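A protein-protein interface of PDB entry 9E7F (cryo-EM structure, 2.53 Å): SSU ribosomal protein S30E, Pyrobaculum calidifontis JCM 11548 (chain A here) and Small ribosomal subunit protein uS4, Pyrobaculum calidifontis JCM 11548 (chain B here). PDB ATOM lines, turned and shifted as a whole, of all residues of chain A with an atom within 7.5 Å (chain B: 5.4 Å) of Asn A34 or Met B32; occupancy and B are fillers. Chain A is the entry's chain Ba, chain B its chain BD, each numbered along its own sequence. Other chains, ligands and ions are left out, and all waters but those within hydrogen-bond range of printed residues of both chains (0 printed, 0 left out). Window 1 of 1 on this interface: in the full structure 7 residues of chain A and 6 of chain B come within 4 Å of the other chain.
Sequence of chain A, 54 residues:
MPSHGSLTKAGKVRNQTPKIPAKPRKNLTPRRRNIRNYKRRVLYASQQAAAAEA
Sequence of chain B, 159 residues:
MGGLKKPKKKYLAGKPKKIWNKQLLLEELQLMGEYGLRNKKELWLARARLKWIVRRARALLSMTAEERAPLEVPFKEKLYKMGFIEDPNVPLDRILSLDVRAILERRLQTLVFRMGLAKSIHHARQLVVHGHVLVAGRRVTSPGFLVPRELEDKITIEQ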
ATOM      1  N   LEU A  28      16.550   5.045   3.862  1.00  0.00           N
ATOM      2  CA  LEU A  28      15.399   5.618   3.191  1.00  0.00           C
ATOM      3  C   LEU A  28      15.432   7.137   3.262  1.00  0.00           C
ATOM      4  O   LEU A  28      16.081   7.735   4.121  1.00  0.00           O
ATOM      5  CB  LEU A  28      14.103   5.102   3.814  1.00  0.00           C
ATOM      6  CG  LEU A  28      14.018   3.600   4.056  1.00  0.00           C
ATOM      7  CD1 LEU A  28      12.595   3.203   4.373  1.00  0.00           C
ATOM      8  CD2 LEU A  28      14.526   2.846   2.850  1.00  0.00           C
ATOM      9  N   THR A  29      14.719   7.758   2.341  1.00  0.00           N
ATOM     10  CA  THR A  29      14.519   9.189   2.397  1.00  0.00           C
ATOM     11  C   THR A  29      13.553   9.524   3.522  1.00  0.00           C
ATOM     12  O   THR A  29      12.894   8.636   4.064  1.00  0.00           O
ATOM     13  CB  THR A  29      13.979   9.700   1.073  1.00  0.00           C
ATOM     14  OG1 THR A  29      12.639   9.231   0.894  1.00  0.00           O
ATOM     15  CG2 THR A  29      14.833   9.192  -0.065  1.00  0.00           C
ATOM     16  N   PRO A  30      13.494  10.797   3.921  1.00  0.00           N
ATOM     17  CA  PRO A  30      12.603  11.190   5.027  1.00  0.00           C
ATOM     18  C   PRO A  30      11.133  10.865   4.815  1.00  0.00           C
ATOM     19  O   PRO A  30      10.440  10.512   5.773  1.00  0.00           O
ATOM     20  CB  PRO A  30      12.838  12.699   5.122  1.00  0.00           C
ATOM     21  CG  PRO A  30      14.200  12.901   4.603  1.00  0.00           C
ATOM     22  CD  PRO A  30      14.453  11.857   3.574  1.00  0.00           C
ATOM     23  N   ARG A  31      10.632  10.972   3.588  1.00  0.00           N
ATOM     24  CA  ARG A  31       9.236  10.630   3.343  1.00  0.00           C
ATOM     25  C   ARG A  31       9.000   9.135   3.493  1.00  0.00           C
ATOM     26  O   ARG A  31       7.985   8.711   4.056  1.00  0.00           O
ATOM     27  CB  ARG A  31       8.818  11.104   1.954  1.00  0.00           C
ATOM     28  CG  ARG A  31       7.452  11.744   1.914  1.00  0.00           C
ATOM     29  CD  ARG A  31       6.985  11.913   0.490  1.00  0.00           C
ATOM     30  NE  ARG A  31       6.834  10.627  -0.177  1.00  0.00           N
ATOM     31  CZ  ARG A  31       7.484  10.272  -1.275  1.00  0.00           C
ATOM     32  NH1 ARG A  31       8.323  11.096  -1.877  1.00  0.00           N
ATOM     33  NH2 ARG A  31       7.290   9.059  -1.778  1.00  0.00           N
ATOM     34  N   ARG A  32       9.931   8.321   2.998  1.00  0.00           N
ATOM     35  CA  ARG A  32       9.748   6.876   3.034  1.00  0.00           C
ATOM     36  C   ARG A  32       9.936   6.315   4.434  1.00  0.00           C
ATOM     37  O   ARG A  32       9.444   5.224   4.733  1.00  0.00           O
ATOM     38  CB  ARG A  32      10.718   6.210   2.068  1.00  0.00           C
ATOM     39  CG  ARG A  32      10.542   6.651   0.637  1.00  0.00           C
ATOM     40  CD  ARG A  32       9.793   5.607  -0.161  1.00  0.00           C
ATOM     41  NE  ARG A  32      10.253   4.257   0.140  1.00  0.00           N
ATOM     42  CZ  ARG A  32       9.452   3.235   0.401  1.00  0.00           C
ATOM     43  NH1 ARG A  32       8.136   3.368   0.394  1.00  0.00           N
ATOM     44  NH2 ARG A  32       9.984   2.048   0.675  1.00  0.00           N
ATOM     45  N   ARG A  33      10.655   7.033   5.296  1.00  0.00           N
ATOM     46  CA  ARG A  33      10.869   6.554   6.656  1.00  0.00           C
ATOM     47  C   ARG A  33       9.573   6.571   7.448  1.00  0.00           C
ATOM     48  O   ARG A  33       9.219   5.588   8.105  1.00  0.00           O
ATOM     49  CB  ARG A  33      11.926   7.410   7.347  1.00  0.00           C
ATOM     50  CG  ARG A  33      12.172   7.063   8.799  1.00  0.00           C
ATOM     51  CD  ARG A  33      12.313   8.307   9.642  1.00  0.00           C
ATOM     52  NE  ARG A  33      12.371   7.995  11.063  1.00  0.00           N
ATOM     53  CZ  ARG A  33      12.242   8.887  12.035  1.00  0.00           C
ATOM     54  NH1 ARG A  33      12.039  10.167  11.777  1.00  0.00           N
ATOM     55  NH2 ARG A  33      12.324   8.486  13.298  1.00  0.00           N
ATOM     56  N   ASN A  34       8.851   7.687   7.399  1.00  0.00           N
ATOM     57  CA  ASN A  34       7.630   7.794   8.184  1.00  0.00           C
ATOM     58  C   ASN A  34       6.498   6.984   7.577  1.00  0.00           C
ATOM     59  O   ASN A  34       5.556   6.616   8.285  1.00  0.00           O
ATOM     60  CB  ASN A  34       7.246   9.258   8.331  1.00  0.00           C
ATOM     61  CG  ASN A  34       8.407  10.098   8.769  1.00  0.00           C
ATOM     62  OD1 ASN A  34       9.505   9.967   8.242  1.00  0.00           O
ATOM     63  ND2 ASN A  34       8.194  10.930   9.770  1.00  0.00           N
ATOM     64  N   ILE A  35       6.565   6.702   6.276  1.00  0.00           N
ATOM     65  CA  ILE A  35       5.659   5.720   5.695  1.00  0.00           C
ATOM     66  C   ILE A  35       5.906   4.355   6.317  1.00  0.00           C
ATOM     67  O   ILE A  35       4.966   3.624   6.649  1.00  0.00           O
ATOM     68  CB  ILE A  35       5.822   5.680   4.168  1.00  0.00           C
ATOM     69  CG1 ILE A  35       4.900   6.697   3.511  1.00  0.00           C
ATOM     70  CG2 ILE A  35       5.529   4.295   3.641  1.00  0.00           C
ATOM     71  CD1 ILE A  35       5.130   6.841   2.036  1.00  0.00           C
ATOM     72  N   ARG A  36       7.178   3.994   6.484  1.00  0.00           N
ATOM     73  CA  ARG A  36       7.522   2.722   7.108  1.00  0.00           C
ATOM     74  C   ARG A  36       7.078   2.685   8.562  1.00  0.00           C
ATOM     75  O   ARG A  36       6.520   1.689   9.029  1.00  0.00           O
ATOM     76  CB  ARG A  36       9.026   2.494   6.998  1.00  0.00           C
ATOM     77  CG  ARG A  36       9.443   1.061   7.191  1.00  0.00           C
ATOM     78  CD  ARG A  36      10.845   0.965   7.748  1.00  0.00           C
ATOM     79  NE  ARG A  36      11.153   2.055   8.661  1.00  0.00           N
ATOM     80  CZ  ARG A  36      12.371   2.531   8.871  1.00  0.00           C
ATOM     81  NH1 ARG A  36      13.421   2.041   8.237  1.00  0.00           N
ATOM     82  NH2 ARG A  36      12.538   3.520   9.740  1.00  0.00           N
ATOM     83  N   ASN A  37       7.310   3.773   9.295  1.00  0.00           N
ATOM     84  CA  ASN A  37       6.974   3.780  10.713  1.00  0.00           C
ATOM     85  C   ASN A  37       5.470   3.813  10.927  1.00  0.00           C
ATOM     86  O   ASN A  37       4.963   3.224  11.887  1.00  0.00           O
ATOM     87  CB  ASN A  37       7.641   4.964  11.401  1.00  0.00           C
ATOM     88  CG  ASN A  37       9.135   4.953  11.234  1.00  0.00           C
ATOM     89  OD1 ASN A  37       9.696   4.035  10.642  1.00  0.00           O
ATOM     90  ND2 ASN A  37       9.794   5.976  11.752  1.00  0.00           N
ATOM     91  N   TYR A  38       4.738   4.505  10.055  1.00  0.00           N
ATOM     92  CA  TYR A  38       3.285   4.499  10.151  1.00  0.00           C
ATOM     93  C   TYR A  38       2.731   3.101   9.916  1.00  0.00           C
ATOM     94  O   TYR A  38       1.810   2.661  10.614  1.00  0.00           O
ATOM     95  CB  TYR A  38       2.687   5.477   9.147  1.00  0.00           C
ATOM     96  CG  TYR A  38       1.196   5.638   9.283  1.00  0.00           C
ATOM     97  CD1 TYR A  38       0.609   5.755  10.526  1.00  0.00           C
ATOM     98  CD2 TYR A  38       0.374   5.650   8.172  1.00  0.00           C
ATOM     99  CE1 TYR A  38      -0.748   5.903  10.659  1.00  0.00           C
ATOM    100  CE2 TYR A  38      -0.989   5.792   8.301  1.00  0.00           C
ATOM    101  CZ  TYR A  38      -1.541   5.916   9.550  1.00  0.00           C
ATOM    102  OH  TYR A  38      -2.897   6.061   9.703  1.00  0.00           O
ATOM    103  N   LYS A  39       3.291   2.384   8.943  1.00  0.00           N
ATOM    104  CA  LYS A  39       2.793   1.055   8.619  1.00  0.00           C
ATOM    105  C   LYS A  39       3.128   0.042   9.703  1.00  0.00           C
ATOM    106  O   LYS A  39       2.396  -0.939   9.875  1.00  0.00           O
ATOM    107  CB  LYS A  39       3.366   0.591   7.281  1.00  0.00           C
ATOM    108  CG  LYS A  39       2.792   1.314   6.080  1.00  0.00           C
ATOM    109  CD  LYS A  39       2.747   0.413   4.861  1.00  0.00           C
ATOM    110  CE  LYS A  39       3.092   1.177   3.596  1.00  0.00           C
ATOM    111  NZ  LYS A  39       4.561   1.265   3.388  1.00  0.00           N
ATOM    112  N   ARG A  40       4.217   0.252  10.439  1.00  0.00           N
ATOM    113  CA  ARG A  40       4.700  -0.766  11.359  1.00  0.00           C
ATOM    114  C   ARG A  40       4.316  -0.517  12.808  1.00  0.00           C
ATOM    115  O   ARG A  40       4.331  -1.461  13.602  1.00  0.00           O
ATOM    116  CB  ARG A  40       6.223  -0.892  11.261  1.00  0.00           C
ATOM    117  CG  ARG A  40       6.670  -2.128  10.513  1.00  0.00           C
ATOM    118  CD  ARG A  40       8.121  -2.451  10.790  1.00  0.00           C
ATOM    119  NE  ARG A  40       8.987  -1.301  10.576  1.00  0.00           N
ATOM    120  CZ  ARG A  40      10.228  -1.205  11.031  1.00  0.00           C
ATOM    121  NH1 ARG A  40      10.775  -2.167  11.752  1.00  0.00           N
ATOM    122  NH2 ARG A  40      10.938  -0.121  10.749  1.00  0.00           N
ATOM    123  N   GLU B  28       2.839  12.145  17.280  1.00  0.00           N
ATOM    124  CA  GLU B  28       3.362  12.783  16.078  1.00  0.00           C
ATOM    125  C   GLU B  28       3.471  11.791  14.929  1.00  0.00           C
ATOM    126  O   GLU B  28       3.251  12.151  13.769  1.00  0.00           O
ATOM    127  CB  GLU B  28       4.715  13.423  16.370  1.00  0.00           C
ATOM    128  CG  GLU B  28       4.657  14.549  17.374  1.00  0.00           C
ATOM    129  CD  GLU B  28       5.741  15.584  17.152  1.00  0.00           C
ATOM    130  OE1 GLU B  28       6.926  15.267  17.377  1.00  0.00           O
ATOM    131  OE2 GLU B  28       5.408  16.718  16.755  1.00  0.00           O
ATOM    132  N   LEU B  29       3.811  10.539  15.231  1.00  0.00           N
ATOM    133  CA  LEU B  29       3.908   9.528  14.185  1.00  0.00           C
ATOM    134  C   LEU B  29       2.551   9.255  13.555  1.00  0.00           C
ATOM    135  O   LEU B  29       2.461   8.929  12.367  1.00  0.00           O
ATOM    136  CB  LEU B  29       4.496   8.243  14.751  1.00  0.00           C
ATOM    137  CG  LEU B  29       4.514   7.058  13.795  1.00  0.00           C
ATOM    138  CD1 LEU B  29       5.138   7.455  12.471  1.00  0.00           C
ATOM    139  CD2 LEU B  29       5.268   5.910  14.422  1.00  0.00           C
ATOM    140  N   GLN B  30       1.484   9.361  14.346  1.00  0.00           N
ATOM    141  CA  GLN B  30       0.137   9.259  13.797  1.00  0.00           C
ATOM    142  C   GLN B  30      -0.137  10.386  12.816  1.00  0.00           C
ATOM    143  O   GLN B  30      -0.692  10.162  11.737  1.00  0.00           O
ATOM    144  CB  GLN B  30      -0.882   9.285  14.929  1.00  0.00           C
ATOM    145  CG  GLN B  30      -2.129   8.493  14.669  1.00  0.00           C
ATOM    146  CD  GLN B  30      -2.689   7.898  15.935  1.00  0.00           C
ATOM    147  OE1 GLN B  30      -1.948   7.378  16.766  1.00  0.00           O
ATOM    148  NE2 GLN B  30      -4.002   7.980  16.098  1.00  0.00           N
ATOM    149  N   LEU B  31       0.259  11.610  13.176  1.00  0.00           N
ATOM    150  CA  LEU B  31      -0.059  12.774  12.357  1.00  0.00           C
ATOM    151  C   LEU B  31       0.656  12.725  11.017  1.00  0.00           C
ATOM    152  O   LEU B  31       0.088  13.110   9.990  1.00  0.00           O
ATOM    153  CB  LEU B  31       0.295  14.053  13.107  1.00  0.00           C
ATOM    154  CG  LEU B  31      -0.798  14.513  14.066  1.00  0.00           C
ATOM    155  CD1 LEU B  31      -0.320  15.636  14.963  1.00  0.00           C
ATOM    156  CD2 LEU B  31      -2.009  14.946  13.276  1.00  0.00           C
ATOM    157  N   MET B  32       1.899  12.248  11.004  1.00  0.00           N
ATOM    158  CA  MET B  32       2.623  12.148   9.744  1.00  0.00           C
ATOM    159  C   MET B  32       2.001  11.091   8.841  1.00  0.00           C
ATOM    160  O   MET B  32       1.987  11.238   7.615  1.00  0.00           O
ATOM    161  CB  MET B  32       4.094  11.835  10.004  1.00  0.00           C
ATOM    162  CG  MET B  32       4.728  12.723  11.055  1.00  0.00           C
ATOM    163  SD  MET B  32       5.600  14.145  10.392  1.00  0.00           S
ATOM    164  CE  MET B  32       6.440  13.417   9.002  1.00  0.00           C
ATOM    165  N   GLY B  33       1.493  10.014   9.429  1.00  0.00           N
ATOM    166  CA  GLY B  33       0.850   8.966   8.666  1.00  0.00           C
ATOM    167  C   GLY B  33      -0.452   9.367   8.007  1.00  0.00           C
ATOM    168  O   GLY B  33      -0.679   9.047   6.837  1.00  0.00           O
ATOM    169  N   GLU B  34      -1.321  10.059   8.750  1.00  0.00           N
ATOM    170  CA  GLU B  34      -2.619  10.450   8.208  1.00  0.00           C
ATOM    171  C   GLU B  34      -2.464  11.426   7.054  1.00  0.00           C
ATOM    172  O   GLU B  34      -3.176  11.331   6.050  1.00  0.00           O
ATOM    173  CB  GLU B  34      -3.485  11.082   9.296  1.00  0.00           C
ATOM    174  CG  GLU B  34      -3.469  10.367  10.628  1.00  0.00           C
ATOM    175  CD  GLU B  34      -4.385  11.014  11.649  1.00  0.00           C
ATOM    176  OE1 GLU B  34      -4.780  12.178  11.440  1.00  0.00           O
ATOM    177  OE2 GLU B  34      -4.704  10.361  12.663  1.00  0.00           O
ATOM    178  N   TYR B  35      -1.541  12.374   7.182  1.00  0.00           N
ATOM    179  CA  TYR B  35      -1.438  13.492   6.258  1.00  0.00           C
ATOM    180  C   TYR B  35      -0.248  13.384   5.320  1.00  0.00           C
ATOM    181  O   TYR B  35      -0.076  14.251   4.460  1.00  0.00           O
ATOM    182  CB  TYR B  35      -1.382  14.800   7.041  1.00  0.00           C
ATOM    183  CG  TYR B  35      -2.634  15.076   7.836  1.00  0.00           C
ATOM    184  CD1 TYR B  35      -2.784  14.592   9.125  1.00  0.00           C
ATOM    185  CD2 TYR B  35      -3.660  15.833   7.302  1.00  0.00           C
ATOM    186  CE1 TYR B  35      -3.925  14.843   9.853  1.00  0.00           C
ATOM    187  CE2 TYR B  35      -4.801  16.093   8.025  1.00  0.00           C
ATOM    188  CZ  TYR B  35      -4.927  15.596   9.299  1.00  0.00           C
ATOM    189  OH  TYR B  35      -6.066  15.853  10.018  1.00  0.00           O
ATOM    190  N   GLY B  36       0.573  12.348   5.457  1.00  0.00           N
ATOM    191  CA  GLY B  36       1.650  12.100   4.520  1.00  0.00           C
ATOM    192  C   GLY B  36       2.712  13.178   4.441  1.00  0.00           C
ATOM    193  O   GLY B  36       3.092  13.598   3.346  1.00  0.00           O
ATOM    194  N   LEU B  37       3.190  13.641   5.588  1.00  0.00           N
ATOM    195  CA  LEU B  37       4.216  14.666   5.602  1.00  0.00           C
ATOM    196  C   LEU B  37       5.584  14.050   5.324  1.00  0.00           C
ATOM    197  O   LEU B  37       5.772  12.834   5.379  1.00  0.00           O
ATOM    198  CB  LEU B  37       4.215  15.394   6.939  1.00  0.00           C
ATOM    199  CG  LEU B  37       2.822  15.617   7.518  1.00  0.00           C
ATOM    200  CD1 LEU B  37       2.924  16.161   8.919  1.00  0.00           C
ATOM    201  CD2 LEU B  37       2.020  16.542   6.637  1.00  0.00           C
ATOM    202  N   ARG B  38       6.551  14.912   5.021  1.00  0.00           N
ATOM    203  CA  ARG B  38       7.885  14.454   4.662  1.00  0.00           C
ATOM    204  C   ARG B  38       8.762  14.212   5.881  1.00  0.00           C
ATOM    205  O   ARG B  38       9.418  13.172   5.979  1.00  0.00           O
ATOM    206  CB  ARG B  38       8.556  15.468   3.744  1.00  0.00           C
ATOM    207  CG  ARG B  38       9.922  15.046   3.274  1.00  0.00           C
ATOM    208  CD  ARG B  38      10.573  16.173   2.509  1.00  0.00           C
ATOM    209  NE  ARG B  38      12.025  16.080   2.500  1.00  0.00           N
ATOM    210  CZ  ARG B  38      12.760  16.145   1.401  1.00  0.00           C
ATOM    211  NH1 ARG B  38      12.205  16.283   0.208  1.00  0.00           N
ATOM    212  NH2 ARG B  38      14.083  16.066   1.498  1.00  0.00           N
ATOM    213  N   ASN B  39       8.796  15.167   6.804  1.00  0.00           N
ATOM    214  CA  ASN B  39       9.596  15.046   8.011  1.00  0.00           C
ATOM    215  C   ASN B  39       8.878  15.759   9.143  1.00  0.00           C
ATOM    216  O   ASN B  39       7.799  16.325   8.964  1.00  0.00           O
ATOM    217  CB  ASN B  39      11.002  15.617   7.816  1.00  0.00           C
ATOM    218  CG  ASN B  39      10.999  16.923   7.073  1.00  0.00           C
ATOM    219  OD1 ASN B  39      10.118  17.755   7.257  1.00  0.00           O
ATOM    220  ND2 ASN B  39      11.994  17.116   6.222  1.00  0.00           N
ATOM    221  N   LYS B  40       9.504  15.742  10.319  1.00  0.00           N
ATOM    222  CA  LYS B  40       8.928  16.417  11.473  1.00  0.00           C
ATOM    223  C   LYS B  40       8.973  17.930  11.341  1.00  0.00           C
ATOM    224  O   LYS B  40       8.251  18.623  12.062  1.00  0.00           O
ATOM    225  CB  LYS B  40       9.655  15.988  12.743  1.00  0.00           C
ATOM    226  CG  LYS B  40       9.654  14.499  12.975  1.00  0.00           C
ATOM    227  CD  LYS B  40       8.266  14.022  13.335  1.00  0.00           C
ATOM    228  CE  LYS B  40       8.288  13.184  14.591  1.00  0.00           C
ATOM    229  NZ  LYS B  40       7.133  12.267  14.678  1.00  0.00           N
ATOM    230  N   LEU B  43       5.624  18.963  10.177  1.00  0.00           N
ATOM    231  CA  LEU B  43       4.674  18.844  11.274  1.00  0.00           C
ATOM    232  C   LEU B  43       4.855  19.960  12.291  1.00  0.00           C
ATOM    233  O   LEU B  43       3.873  20.509  12.803  1.00  0.00           O
ATOM    234  CB  LEU B  43       4.824  17.482  11.941  1.00  0.00           C
ATOM    235  CG  LEU B  43       3.915  17.224  13.137  1.00  0.00           C
ATOM    236  CD1 LEU B  43       2.478  17.530  12.783  1.00  0.00           C
ATOM    237  CD2 LEU B  43       4.062  15.793  13.594  1.00  0.00           C
ATOM    238  N   HIS B 122      -0.288   9.992  -0.390  1.00  0.00           N
ATOM    239  CA  HIS B 122       1.029  10.091  -0.997  1.00  0.00           C
ATOM    240  C   HIS B 122       0.944  10.206  -2.507  1.00  0.00           C
ATOM    241  O   HIS B 122       1.849  10.767  -3.129  1.00  0.00           O
ATOM    242  CB  HIS B 122       1.872   8.888  -0.590  1.00  0.00           C
ATOM    243  CG  HIS B 122       2.149   8.828   0.878  1.00  0.00           C
ATOM    244  ND1 HIS B 122       2.957   9.741   1.520  1.00  0.00           N
ATOM    245  CD2 HIS B 122       1.705   7.980   1.835  1.00  0.00           C
ATOM    246  CE1 HIS B 122       3.012   9.449   2.806  1.00  0.00           C
ATOM    247  NE2 HIS B 122       2.259   8.387   3.024  1.00  0.00           N
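The guanidinium group of Arg A36 lies within hydrogen-bond range of the side-chain amide oxygen of Asn A37 (3.0 Å). The backbone carbonyl oxygen (O) of Met B32 lies within hydrogen-bond range of the backbone NH (N) of Leu B37 (3.4 Å). The side-chain amide oxygen (OD1) of Asn A34 sits close to the backbone carbonyl oxygen (O) of Pro A30, 2.7 Å away. O of Arg A33 sits close to OD1 of Asn A37 (3.0 Å).
Among the printed residues, merely in contact across the chains: Asn A34 with Met B32, Asn A34 with Arg B38, Ile A35 with His B122, Asn A37 with Leu B29, Tyr A38 with Leu B29 and Tyr A38 with Gly B33.
Asn A34 touches just these residues of chain B: Met B32 and Arg B38. Of the printed residues of chain B, Asn A37 touches Leu B29 (3.7 Å). Of the printed residues of chain B, Tyr A38 touches Leu B29 and Gly B33. Met B32 touches just one residue of chain A: Asn A34. Printed residues of chain A within 4 Å of His B122: Ile A35. The nearest residue of chain A that does not touch Met B32 is Tyr A38 (5.5 Å). The nearest printed residue of chain B that does not touch Ile A35 is Leu B37 (6.2 Å).
The backbone carbonyl oxygen (O) of Arg B38 lies within hydrogen-bond range of the backbone NH (N) of Arg A31, 3.5 Å away. O of Pro A30 lies close to O of Arg B38 (2.9 Å).
Hydrophobic or aromatic side chains of chain B within 4 Å of the printed part of chain A: Leu B29, Met B32 and His B122. Printed residues of chain A that touch a printed residue of chain B: Pro A30, Arg A31, Asn A34, Ile A35, Asn A37 and Tyr A38. Among the printed residues, 8 pairs touch across the chains. Among the printed residues, no Asp or Glu carboxylate lies within 4 Å of a Lys or Arg side-chain nitrogen of the other chain.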
